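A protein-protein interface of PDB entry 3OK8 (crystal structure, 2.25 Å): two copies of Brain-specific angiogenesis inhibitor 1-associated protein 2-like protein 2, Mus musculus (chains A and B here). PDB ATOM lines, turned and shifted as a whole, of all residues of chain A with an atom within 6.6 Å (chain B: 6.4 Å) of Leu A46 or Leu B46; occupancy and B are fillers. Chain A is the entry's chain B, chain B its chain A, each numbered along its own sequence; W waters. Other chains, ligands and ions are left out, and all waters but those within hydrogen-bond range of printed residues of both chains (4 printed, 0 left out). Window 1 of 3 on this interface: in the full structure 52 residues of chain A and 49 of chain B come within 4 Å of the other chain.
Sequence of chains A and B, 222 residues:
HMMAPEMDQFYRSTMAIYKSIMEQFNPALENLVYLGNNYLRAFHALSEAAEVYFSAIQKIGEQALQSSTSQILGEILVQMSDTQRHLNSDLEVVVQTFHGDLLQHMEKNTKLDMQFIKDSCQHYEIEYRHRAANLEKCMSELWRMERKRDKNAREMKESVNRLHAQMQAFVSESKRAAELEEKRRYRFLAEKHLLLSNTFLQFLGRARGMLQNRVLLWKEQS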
ATOM      1  N   ASN A  38      -2.829   2.971  17.744  1.00  0.00           N
ATOM      2  CA  ASN A  38      -3.031   1.540  17.576  1.00  0.00           C
ATOM      3  C   ASN A  38      -3.884   1.309  16.338  1.00  0.00           C
ATOM      4  O   ASN A  38      -3.587   0.447  15.514  1.00  0.00           O
ATOM      5  CB  ASN A  38      -3.728   0.940  18.786  1.00  0.00           C
ATOM      6  CG  ASN A  38      -3.984  -0.543  18.633  1.00  0.00           C
ATOM      7  OD1 ASN A  38      -3.154  -1.281  18.088  1.00  0.00           O
ATOM      8  ND2 ASN A  38      -5.128  -0.999  19.136  1.00  0.00           N
ATOM      9  N   TYR A  39      -4.941   2.097  16.218  1.00  0.00           N
ATOM     10  CA  TYR A  39      -5.827   2.076  15.066  1.00  0.00           C
ATOM     11  C   TYR A  39      -5.049   2.312  13.769  1.00  0.00           C
ATOM     12  O   TYR A  39      -5.213   1.576  12.785  1.00  0.00           O
ATOM     13  CB  TYR A  39      -6.862   3.183  15.234  1.00  0.00           C
ATOM     14  CG  TYR A  39      -8.123   3.011  14.438  1.00  0.00           C
ATOM     15  CD1 TYR A  39      -9.324   3.496  14.931  1.00  0.00           C
ATOM     16  CD2 TYR A  39      -8.124   2.373  13.194  1.00  0.00           C
ATOM     17  CE1 TYR A  39     -10.500   3.358  14.220  1.00  0.00           C
ATOM     18  CE2 TYR A  39      -9.303   2.218  12.470  1.00  0.00           C
ATOM     19  CZ  TYR A  39     -10.491   2.718  12.995  1.00  0.00           C
ATOM     20  OH  TYR A  39     -11.684   2.595  12.314  1.00  0.00           O
ATOM     21  N   LEU A  40      -4.228   3.361  13.769  1.00  0.00           N
ATOM     22  CA  LEU A  40      -3.392   3.704  12.618  1.00  0.00           C
ATOM     23  C   LEU A  40      -2.483   2.546  12.258  1.00  0.00           C
ATOM     24  O   LEU A  40      -2.261   2.240  11.083  1.00  0.00           O
ATOM     25  CB  LEU A  40      -2.545   4.945  12.928  1.00  0.00           C
ATOM     26  CG  LEU A  40      -2.904   6.270  12.242  1.00  0.00           C
ATOM     27  CD1 LEU A  40      -4.409   6.400  12.020  1.00  0.00           C
ATOM     28  CD2 LEU A  40      -2.340   7.477  13.000  1.00  0.00           C
ATOM     29  N   ARG A  41      -1.961   1.900  13.291  1.00  0.00           N
ATOM     30  CA  ARG A  41      -1.061   0.773  13.123  1.00  0.00           C
ATOM     31  C   ARG A  41      -1.766  -0.401  12.431  1.00  0.00           C
ATOM     32  O   ARG A  41      -1.219  -1.002  11.528  1.00  0.00           O
ATOM     33  CB  ARG A  41      -0.478   0.359  14.481  1.00  0.00           C
ATOM     34  CG  ARG A  41       0.552  -0.750  14.419  1.00  0.00           C
ATOM     35  CD  ARG A  41       1.216  -0.942  15.762  1.00  0.00           C
ATOM     36  NE  ARG A  41       0.255  -1.332  16.793  1.00  0.00           N
ATOM     37  CZ  ARG A  41       0.588  -1.595  18.055  1.00  0.00           C
ATOM     38  NH1 ARG A  41      -0.341  -1.945  18.940  1.00  0.00           N
ATOM     39  NH2 ARG A  41       1.858  -1.518  18.430  1.00  0.00           N
ATOM     40  N   ALA A  42      -2.991  -0.710  12.834  1.00  0.00           N
ATOM     41  CA  ALA A  42      -3.707  -1.820  12.212  1.00  0.00           C
ATOM     42  C   ALA A  42      -4.111  -1.521  10.757  1.00  0.00           C
ATOM     43  O   ALA A  42      -4.168  -2.435   9.906  1.00  0.00           O
ATOM     44  CB  ALA A  42      -4.905  -2.207  13.036  1.00  0.00           C
ATOM     45  N   PHE A  43      -4.382  -0.251  10.466  1.00  0.00           N
ATOM     46  CA  PHE A  43      -4.679   0.149   9.101  1.00  0.00           C
ATOM     47  C   PHE A  43      -3.497  -0.019   8.156  1.00  0.00           C
ATOM     48  O   PHE A  43      -3.663  -0.521   7.045  1.00  0.00           O
ATOM     49  CB  PHE A  43      -5.171   1.589   9.003  1.00  0.00           C
ATOM     50  CG  PHE A  43      -5.302   2.058   7.582  1.00  0.00           C
ATOM     51  CD1 PHE A  43      -4.213   2.621   6.918  1.00  0.00           C
ATOM     52  CD2 PHE A  43      -6.487   1.874   6.881  1.00  0.00           C
ATOM     53  CE1 PHE A  43      -4.311   3.024   5.589  1.00  0.00           C
ATOM     54  CE2 PHE A  43      -6.598   2.275   5.550  1.00  0.00           C
ATOM     55  CZ  PHE A  43      -5.509   2.857   4.906  1.00  0.00           C
ATOM     56  N   HIS A  44      -2.316   0.436   8.562  1.00  0.00           N
ATOM     57  CA  HIS A  44      -1.149   0.309   7.692  1.00  0.00           C
ATOM     58  C   HIS A  44      -0.732  -1.150   7.491  1.00  0.00           C
ATOM     59  O   HIS A  44      -0.032  -1.482   6.520  1.00  0.00           O
ATOM     60  CB  HIS A  44       0.030   1.152   8.191  1.00  0.00           C
ATOM     61  CG  HIS A  44      -0.247   2.625   8.214  1.00  0.00           C
ATOM     62  ND1 HIS A  44       0.082   3.430   9.285  1.00  0.00           N
ATOM     63  CD2 HIS A  44      -0.835   3.436   7.303  1.00  0.00           C
ATOM     64  CE1 HIS A  44      -0.288   4.673   9.029  1.00  0.00           C
ATOM     65  NE2 HIS A  44      -0.849   4.704   7.833  1.00  0.00           N
ATOM     66  N   ALA A  45      -1.169  -2.013   8.405  1.00  0.00           N
ATOM     67  CA  ALA A  45      -0.920  -3.446   8.285  1.00  0.00           C
ATOM     68  C   ALA A  45      -1.906  -4.108   7.315  1.00  0.00           C
ATOM     69  O   ALA A  45      -1.530  -4.980   6.542  1.00  0.00           O
ATOM     70  CB  ALA A  45      -0.982  -4.107   9.653  1.00  0.00           C
ATOM     71  N   LEU A  46      -3.166  -3.690   7.375  1.00  0.00           N
ATOM     72  CA  LEU A  46      -4.202  -4.119   6.449  1.00  0.00           C
ATOM     73  C   LEU A  46      -3.796  -3.703   5.042  1.00  0.00           C
ATOM     74  O   LEU A  46      -3.888  -4.482   4.090  1.00  0.00           O
ATOM     75  CB  LEU A  46      -5.517  -3.425   6.801  1.00  0.00           C
ATOM     76  CG  LEU A  46      -6.858  -4.144   6.645  1.00  0.00           C
ATOM     77  CD1 LEU A  46      -7.954  -3.113   6.493  1.00  0.00           C
ATOM     78  CD2 LEU A  46      -6.887  -5.106   5.496  1.00  0.00           C
ATOM     79  N   SER A  47      -3.364  -2.452   4.919  1.00  0.00           N
ATOM     80  CA  SER A  47      -2.866  -1.917   3.664  1.00  0.00           C
ATOM     81  C   SER A  47      -1.788  -2.829   3.090  1.00  0.00           C
ATOM     82  O   SER A  47      -1.826  -3.200   1.923  1.00  0.00           O
ATOM     83  CB  SER A  47      -2.287  -0.525   3.908  1.00  0.00           C
ATOM     84  OG  SER A  47      -1.700   0.002   2.739  1.00  0.00           O
ATOM     85  N   GLU A  48      -0.822  -3.173   3.939  1.00  0.00           N
ATOM     86  CA  GLU A  48       0.283  -4.021   3.519  1.00  0.00           C
ATOM     87  C   GLU A  48      -0.158  -5.423   3.127  1.00  0.00           C
ATOM     88  O   GLU A  48       0.345  -5.958   2.147  1.00  0.00           O
ATOM     89  CB  GLU A  48       1.389  -4.068   4.570  1.00  0.00           C
ATOM     90  CG  GLU A  48       2.039  -2.718   4.816  1.00  0.00           C
ATOM     91  CD  GLU A  48       2.271  -1.919   3.538  1.00  0.00           C
ATOM     92  OE1 GLU A  48       3.452  -1.618   3.250  1.00  0.00           O
ATOM     93  OE2 GLU A  48       1.285  -1.585   2.829  1.00  0.00           O
ATOM     94  N   ALA A  49      -1.097  -5.999   3.871  1.00  0.00           N
ATOM     95  CA  ALA A  49      -1.654  -7.295   3.537  1.00  0.00           C
ATOM     96  C   ALA A  49      -2.335  -7.231   2.168  1.00  0.00           C
ATOM     97  O   ALA A  49      -2.050  -8.042   1.296  1.00  0.00           O
ATOM     98  CB  ALA A  49      -2.642  -7.748   4.610  1.00  0.00           C
ATOM     99  N   ALA A  50      -3.222  -6.253   1.989  1.00  0.00           N
ATOM    100  CA  ALA A  50      -3.997  -6.107   0.761  1.00  0.00           C
ATOM    101  C   ALA A  50      -3.105  -5.870  -0.439  1.00  0.00           C
ATOM    102  O   ALA A  50      -3.394  -6.317  -1.551  1.00  0.00           O
ATOM    103  CB  ALA A  50      -4.964  -4.952   0.902  1.00  0.00           C
ATOM    104  N   GLU A  51      -2.032  -5.140  -0.188  1.00  0.00           N
ATOM    105  CA  GLU A  51      -1.054  -4.750  -1.192  1.00  0.00           C
ATOM    106  C   GLU A  51      -0.326  -5.983  -1.705  1.00  0.00           C
ATOM    107  O   GLU A  51      -0.094  -6.151  -2.902  1.00  0.00           O
ATOM    108  CB  GLU A  51      -0.039  -3.809  -0.542  1.00  0.00           C
ATOM    109  CG  GLU A  51       0.771  -2.951  -1.495  1.00  0.00           C
ATOM    110  CD  GLU A  51       0.905  -3.569  -2.858  1.00  0.00           C
ATOM    111  OE1 GLU A  51      -0.057  -3.453  -3.652  1.00  0.00           O
ATOM    112  OE2 GLU A  51       1.969  -4.166  -3.135  1.00  0.00           O
ATOM    113  N   GLN A  84      -7.384  -1.664  -6.723  1.00  0.00           N
ATOM    114  CA  GLN A  84      -7.073  -1.771  -5.296  1.00  0.00           C
ATOM    115  C   GLN A  84      -5.960  -0.797  -4.886  1.00  0.00           C
ATOM    116  O   GLN A  84      -6.076  -0.083  -3.895  1.00  0.00           O
ATOM    117  CB  GLN A  84      -6.690  -3.212  -4.940  1.00  0.00           C
ATOM    118  CG  GLN A  84      -6.415  -3.453  -3.476  1.00  0.00           C
ATOM    119  CD  GLN A  84      -4.990  -3.127  -3.097  1.00  0.00           C
ATOM    120  OE1 GLN A  84      -4.130  -2.944  -3.963  1.00  0.00           O
ATOM    121  NE2 GLN A  84      -4.724  -3.062  -1.798  1.00  0.00           N
ATOM    122  N   ASN A  88      -6.412   2.140  -2.196  1.00  0.00           N
ATOM    123  CA  ASN A  88      -5.519   2.214  -1.037  1.00  0.00           C
ATOM    124  C   ASN A  88      -4.818   3.560  -0.945  1.00  0.00           C
ATOM    125  O   ASN A  88      -4.721   4.172   0.119  1.00  0.00           O
ATOM    126  CB  ASN A  88      -4.439   1.140  -1.115  1.00  0.00           C
ATOM    127  CG  ASN A  88      -4.915  -0.216  -0.648  1.00  0.00           C
ATOM    128  OD1 ASN A  88      -4.115  -1.039  -0.191  1.00  0.00           O
ATOM    129  ND2 ASN A  88      -6.215  -0.465  -0.765  1.00  0.00           N
ATOM    130  N   TYR B  39      -4.531 -11.341   4.953  1.00  0.00           N
ATOM    131  CA  TYR B  39      -5.437 -10.234   4.670  1.00  0.00           C
ATOM    132  C   TYR B  39      -6.626 -10.202   5.656  1.00  0.00           C
ATOM    133  O   TYR B  39      -6.965  -9.154   6.212  1.00  0.00           O
ATOM    134  CB  TYR B  39      -5.935 -10.391   3.238  1.00  0.00           C
ATOM    135  CG  TYR B  39      -6.434  -9.137   2.561  1.00  0.00           C
ATOM    136  CD1 TYR B  39      -6.727  -7.987   3.279  1.00  0.00           C
ATOM    137  CD2 TYR B  39      -6.648  -9.122   1.190  1.00  0.00           C
ATOM    138  CE1 TYR B  39      -7.195  -6.849   2.638  1.00  0.00           C
ATOM    139  CE2 TYR B  39      -7.119  -7.998   0.547  1.00  0.00           C
ATOM    140  CZ  TYR B  39      -7.397  -6.866   1.269  1.00  0.00           C
ATOM    141  OH  TYR B  39      -7.864  -5.753   0.597  1.00  0.00           O
ATOM    142  N   LEU B  40      -7.258 -11.352   5.872  1.00  0.00           N
ATOM    143  CA  LEU B  40      -8.377 -11.444   6.806  1.00  0.00           C
ATOM    144  C   LEU B  40      -7.946 -11.069   8.213  1.00  0.00           C
ATOM    145  O   LEU B  40      -8.624 -10.300   8.892  1.00  0.00           O
ATOM    146  CB  LEU B  40      -8.953 -12.859   6.843  1.00  0.00           C
ATOM    147  CG  LEU B  40      -9.836 -13.296   5.684  1.00  0.00           C
ATOM    148  CD1 LEU B  40      -9.931 -14.820   5.648  1.00  0.00           C
ATOM    149  CD2 LEU B  40     -11.202 -12.662   5.814  1.00  0.00           C
ATOM    150  N   ARG B  41      -6.832 -11.637   8.660  1.00  0.00           N
ATOM    151  CA  ARG B  41      -6.337 -11.370  10.004  1.00  0.00           C
ATOM    152  C   ARG B  41      -6.046  -9.883  10.211  1.00  0.00           C
ATOM    153  O   ARG B  41      -6.354  -9.338  11.265  1.00  0.00           O
ATOM    154  CB  ARG B  41      -5.125 -12.248  10.343  1.00  0.00           C
ATOM    155  CG  ARG B  41      -5.495 -13.705  10.646  1.00  0.00           C
ATOM    156  CD  ARG B  41      -4.284 -14.542  11.086  1.00  0.00           C
ATOM    157  NE  ARG B  41      -3.355 -14.788   9.987  1.00  0.00           N
ATOM    158  CZ  ARG B  41      -3.352 -15.885   9.228  1.00  0.00           C
ATOM    159  NH1 ARG B  41      -4.220 -16.864   9.447  1.00  0.00           N
ATOM    160  NH2 ARG B  41      -2.466 -16.013   8.247  1.00  0.00           N
ATOM    161  N   ALA B  42      -5.474  -9.218   9.210  1.00  0.00           N
ATOM    162  CA  ALA B  42      -5.319  -7.764   9.282  1.00  0.00           C
ATOM    163  C   ALA B  42      -6.660  -7.069   9.414  1.00  0.00           C
ATOM    164  O   ALA B  42      -6.795  -6.156  10.225  1.00  0.00           O
ATOM    165  CB  ALA B  42      -4.562  -7.219   8.086  1.00  0.00           C
ATOM    166  N   PHE B  43      -7.640  -7.481   8.602  1.00  0.00           N
ATOM    167  CA  PHE B  43      -9.007  -6.967   8.707  1.00  0.00           C
ATOM    168  C   PHE B  43      -9.573  -7.111  10.116  1.00  0.00           C
ATOM    169  O   PHE B  43     -10.166  -6.181  10.649  1.00  0.00           O
ATOM    170  CB  PHE B  43      -9.954  -7.722   7.773  1.00  0.00           C
ATOM    171  CG  PHE B  43     -10.125  -7.100   6.413  1.00  0.00           C
ATOM    172  CD1 PHE B  43     -10.770  -5.875   6.267  1.00  0.00           C
ATOM    173  CD2 PHE B  43      -9.693  -7.773   5.271  1.00  0.00           C
ATOM    174  CE1 PHE B  43     -10.951  -5.311   5.000  1.00  0.00           C
ATOM    175  CE2 PHE B  43      -9.869  -7.222   4.000  1.00  0.00           C
ATOM    176  CZ  PHE B  43     -10.493  -5.985   3.865  1.00  0.00           C
ATOM    177  N   HIS B  44      -9.439  -8.298  10.694  1.00  0.00           N
ATOM    178  CA  HIS B  44     -10.025  -8.570  11.999  1.00  0.00           C
ATOM    179  C   HIS B  44      -9.354  -7.718  13.084  1.00  0.00           C
ATOM    180  O   HIS B  44      -9.986  -7.323  14.062  1.00  0.00           O
ATOM    181  CB  HIS B  44      -9.901 -10.061  12.341  1.00  0.00           C
ATOM    182  CG  HIS B  44     -10.752 -10.962  11.496  1.00  0.00           C
ATOM    183  ND1 HIS B  44     -12.099 -10.740  11.281  1.00  0.00           N
ATOM    184  CD2 HIS B  44     -10.452 -12.104  10.834  1.00  0.00           C
ATOM    185  CE1 HIS B  44     -12.584 -11.701  10.518  1.00  0.00           C
ATOM    186  NE2 HIS B  44     -11.604 -12.541  10.229  1.00  0.00           N
ATOM    187  N   ALA B  45      -8.064  -7.459  12.896  1.00  0.00           N
ATOM    188  CA  ALA B  45      -7.289  -6.612  13.795  1.00  0.00           C
ATOM    189  C   ALA B  45      -7.685  -5.140  13.666  1.00  0.00           C
ATOM    190  O   ALA B  45      -7.722  -4.415  14.665  1.00  0.00           O
ATOM    191  CB  ALA B  45      -5.792  -6.789  13.543  1.00  0.00           C
ATOM    192  N   LEU B  46      -7.961  -4.688  12.440  1.00  0.00           N
ATOM    193  CA  LEU B  46      -8.386  -3.301  12.255  1.00  0.00           C
ATOM    194  C   LEU B  46      -9.736  -3.095  12.917  1.00  0.00           C
ATOM    195  O   LEU B  46      -9.933  -2.127  13.636  1.00  0.00           O
ATOM    196  CB  LEU B  46      -8.465  -2.902  10.783  1.00  0.00           C
ATOM    197  CG  LEU B  46      -8.869  -1.443  10.518  1.00  0.00           C
ATOM    198  CD1 LEU B  46      -7.734  -0.457  10.846  1.00  0.00           C
ATOM    199  CD2 LEU B  46      -9.296  -1.261   9.093  1.00  0.00           C
ATOM    200  N   SER B  47     -10.661  -4.018  12.689  1.00  0.00           N
ATOM    201  CA  SER B  47     -11.990  -3.861  13.247  1.00  0.00           C
ATOM    202  C   SER B  47     -11.960  -3.833  14.788  1.00  0.00           C
ATOM    203  O   SER B  47     -12.822  -3.218  15.407  1.00  0.00           O
ATOM    204  CB  SER B  47     -12.946  -4.937  12.713  1.00  0.00           C
ATOM    205  OG  SER B  47     -12.890  -6.114  13.495  1.00  0.00           O
ATOM    206  N   GLU B  48     -10.963  -4.473  15.397  1.00  0.00           N
ATOM    207  CA  GLU B  48     -10.828  -4.486  16.852  1.00  0.00           C
ATOM    208  C   GLU B  48     -10.337  -3.136  17.389  1.00  0.00           C
ATOM    209  O   GLU B  48     -10.977  -2.537  18.240  1.00  0.00           O
ATOM    210  CB  GLU B  48      -9.892  -5.611  17.298  1.00  0.00           C
ATOM    211  CG  GLU B  48     -10.616  -6.773  17.959  1.00  0.00           C
ATOM    212  CD  GLU B  48     -10.952  -6.499  19.426  1.00  0.00           C
ATOM    213  OE1 GLU B  48     -10.128  -5.873  20.123  1.00  0.00           O
ATOM    214  OE2 GLU B  48     -12.036  -6.922  19.881  1.00  0.00           O
ATOM    215  N   ALA B  49      -9.203  -2.680  16.867  1.00  0.00           N
ATOM    216  CA  ALA B  49      -8.660  -1.363  17.138  1.00  0.00           C
ATOM    217  C   ALA B  49      -9.684  -0.258  16.946  1.00  0.00           C
ATOM    218  O   ALA B  49      -9.646   0.730  17.663  1.00  0.00           O
ATOM    219  CB  ALA B  49      -7.468  -1.104  16.251  1.00  0.00           C
ATOM    220  N   ALA B  50     -10.575  -0.409  15.970  1.00  0.00           N
ATOM    221  CA  ALA B  50     -11.640   0.568  15.755  1.00  0.00           C
ATOM    222  C   ALA B  50     -12.673   0.487  16.861  1.00  0.00           C
ATOM    223  O   ALA B  50     -13.080   1.504  17.407  1.00  0.00           O
ATOM    224  CB  ALA B  50     -12.314   0.362  14.398  1.00  0.00           C
ATOM    225  N   GLU B  51     -13.099  -0.727  17.189  1.00  0.00           N
ATOM    226  CA  GLU B  51     -14.106  -0.914  18.214  1.00  0.00           C
ATOM    227  C   GLU B  51     -13.646  -0.404  19.590  1.00  0.00           C
ATOM    228  O   GLU B  51     -14.447   0.143  20.350  1.00  0.00           O
ATOM    229  CB  GLU B  51     -14.519  -2.385  18.268  1.00  0.00           C
ATOM    230  CG  GLU B  51     -15.529  -2.724  19.352  1.00  0.00           C
ATOM    231  CD  GLU B  51     -16.949  -2.281  19.019  1.00  0.00           C
ATOM    232  OE1 GLU B  51     -17.282  -2.147  17.815  1.00  0.00           O
ATOM    233  OE2 GLU B  51     -17.738  -2.083  19.971  1.00  0.00           O
ATOM    234  N   ASN B  88     -18.961  -1.089  10.561  1.00  0.00           N
ATOM    235  CA  ASN B  88     -18.160  -2.276  10.791  1.00  0.00           C
ATOM    236  C   ASN B  88     -18.969  -3.538  10.592  1.00  0.00           C
ATOM    237  O   ASN B  88     -18.449  -4.543  10.100  1.00  0.00           O
ATOM    238  CB  ASN B  88     -17.577  -2.277  12.198  1.00  0.00           C
ATOM    239  CG  ASN B  88     -16.627  -3.431  12.426  1.00  0.00           C
ATOM    240  OD1 ASN B  88     -16.919  -4.357  13.187  1.00  0.00           O
ATOM    241  ND2 ASN B  88     -15.485  -3.391  11.757  1.00  0.00           N
ATOM    242  N   LEU B  91     -19.090  -3.952   7.026  1.00  0.00           N
ATOM    243  CA  LEU B  91     -17.843  -4.349   6.415  1.00  0.00           C
ATOM    244  C   LEU B  91     -17.504  -5.811   6.682  1.00  0.00           C
ATOM    245  O   LEU B  91     -16.929  -6.471   5.822  1.00  0.00           O
ATOM    246  CB  LEU B  91     -16.692  -3.434   6.822  1.00  0.00           C
ATOM    247  CG  LEU B  91     -15.394  -3.775   6.071  1.00  0.00           C
ATOM    248  CD1 LEU B  91     -15.490  -3.349   4.608  1.00  0.00           C
ATOM    249  CD2 LEU B  91     -14.159  -3.178   6.740  1.00  0.00           C
HETATM  250  O   HOH W   1      -7.196   1.168  18.926  1.00  0.00           O
HETATM  251  O   HOH W   2      -4.407  -4.821  10.785  1.00  0.00           O
HETATM  252  O   HOH W   3      -7.211  -2.741   1.262  1.00  0.00           O
HETATM  253  O   HOH W   4      -7.199  -3.406  19.569  1.00  0.00           O
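OD1 of Asn A38 lies within hydrogen-bond range of NH1 of Arg A41 (3.0 Å).
Among the printed residues, pairs that only touch across the chains: Asn A38 with Ala B49 (3.7 Å), Tyr A39 with Leu B46 (3.5 Å), Tyr A39 with Ala B49 (3.8 Å), Tyr A39 with Ala B50 (3.1 Å), Ala A42 with Ala B45 (3.9 Å), Ala A42 with Leu B46 (3.7 Å), Phe A43 with Leu B46 (3.4 Å), Leu A46 with Tyr B39 (3.4 Å), Leu A46 with Ala B42 (3.5 Å), Leu A46 with Phe B43 (3.9 Å), Leu A46 with Leu B46 (3.5 Å), Ala A49 with Tyr B39 (3.7 Å) and Ala A50 with Tyr B39 (3.0 Å).
Of the printed residues of chain A, Leu B46 touches Tyr A39 (3.5 Å), Ala A42 (3.7 Å), Phe A43 (3.4 Å) and Leu A46 (3.5 Å).
Printed residues of chain B within 4 Å of Ala A49: Tyr B39 (3.7 Å).
Of the printed residues of chain B, Ala A42 touches Ala B45 and Leu B46.
Of the printed residues of chain B, Phe A43 touches Leu B46.
Ser A47 touches none of the printed residues of chain B.
The nearest residue of chain B that does not touch Leu A46 is Leu B91 (6.2 Å).
The nearest printed residue of chain A that does not touch Leu B46 is His A44 (5.9 Å).
Of the 16 printed residues of chain A, 7 touch a printed residue of chain B.
Of the 15 printed residues of chain B, 7 touch a printed residue of chain A.
Hydrophobic or aromatic side chains of chain B that line the printed part of chain A: Tyr B39, Ala B42, Phe B43, Leu B46, Ala B49 and Ala B50.
Among the printed residues, 13 pairs touch across the chains.
Among the printed residues, no Asp or Glu carboxylate lies within 4 Å of a Lys or Arg side-chain nitrogen of the other chain.
Tyr A39 touches Ala B49, and with the chains exchanged Ala A49 touches Tyr B39.
Ala A42 touches Ala B45, but with the chains exchanged Ala A45 does not touch Ala B42 (4.1 Å).
Ala A42 touches Leu B46, and with the chains exchanged Leu A46 touches Ala B42.
Phe A43 touches Leu B46, and with the chains exchanged Leu A46 touches Phe B43.
Positions printed for both chains: 39, 40, 41, 42, 43, 44, 45, 46, 47, 48, 49, 50, 51 and 88.
Of the 13 pairs that touch across the chains among the printed residues, 11 have their exchanged pair printed and touching as well.
Water W2 bridges the backbone carbonyl oxygen (O) of Ala A42 (2.6 Å) and the backbone carbonyl oxygen (O) of Ala B42 (2.8 Å).
Water W1 bridges O of Ala B49 (2.8 Å) and ND2 of Asn A38 (3.0 Å).
Water W3 bridges the side-chain hydroxyl (OH) of Tyr B39 (3.2 Å) and the side-chain amide nitrogen (ND2) of Asn A88 (3.2 Å).
Water W4 bridges ND2 of Asn A38 (3.2 Å) and N of Ala B49 (3.4 Å).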
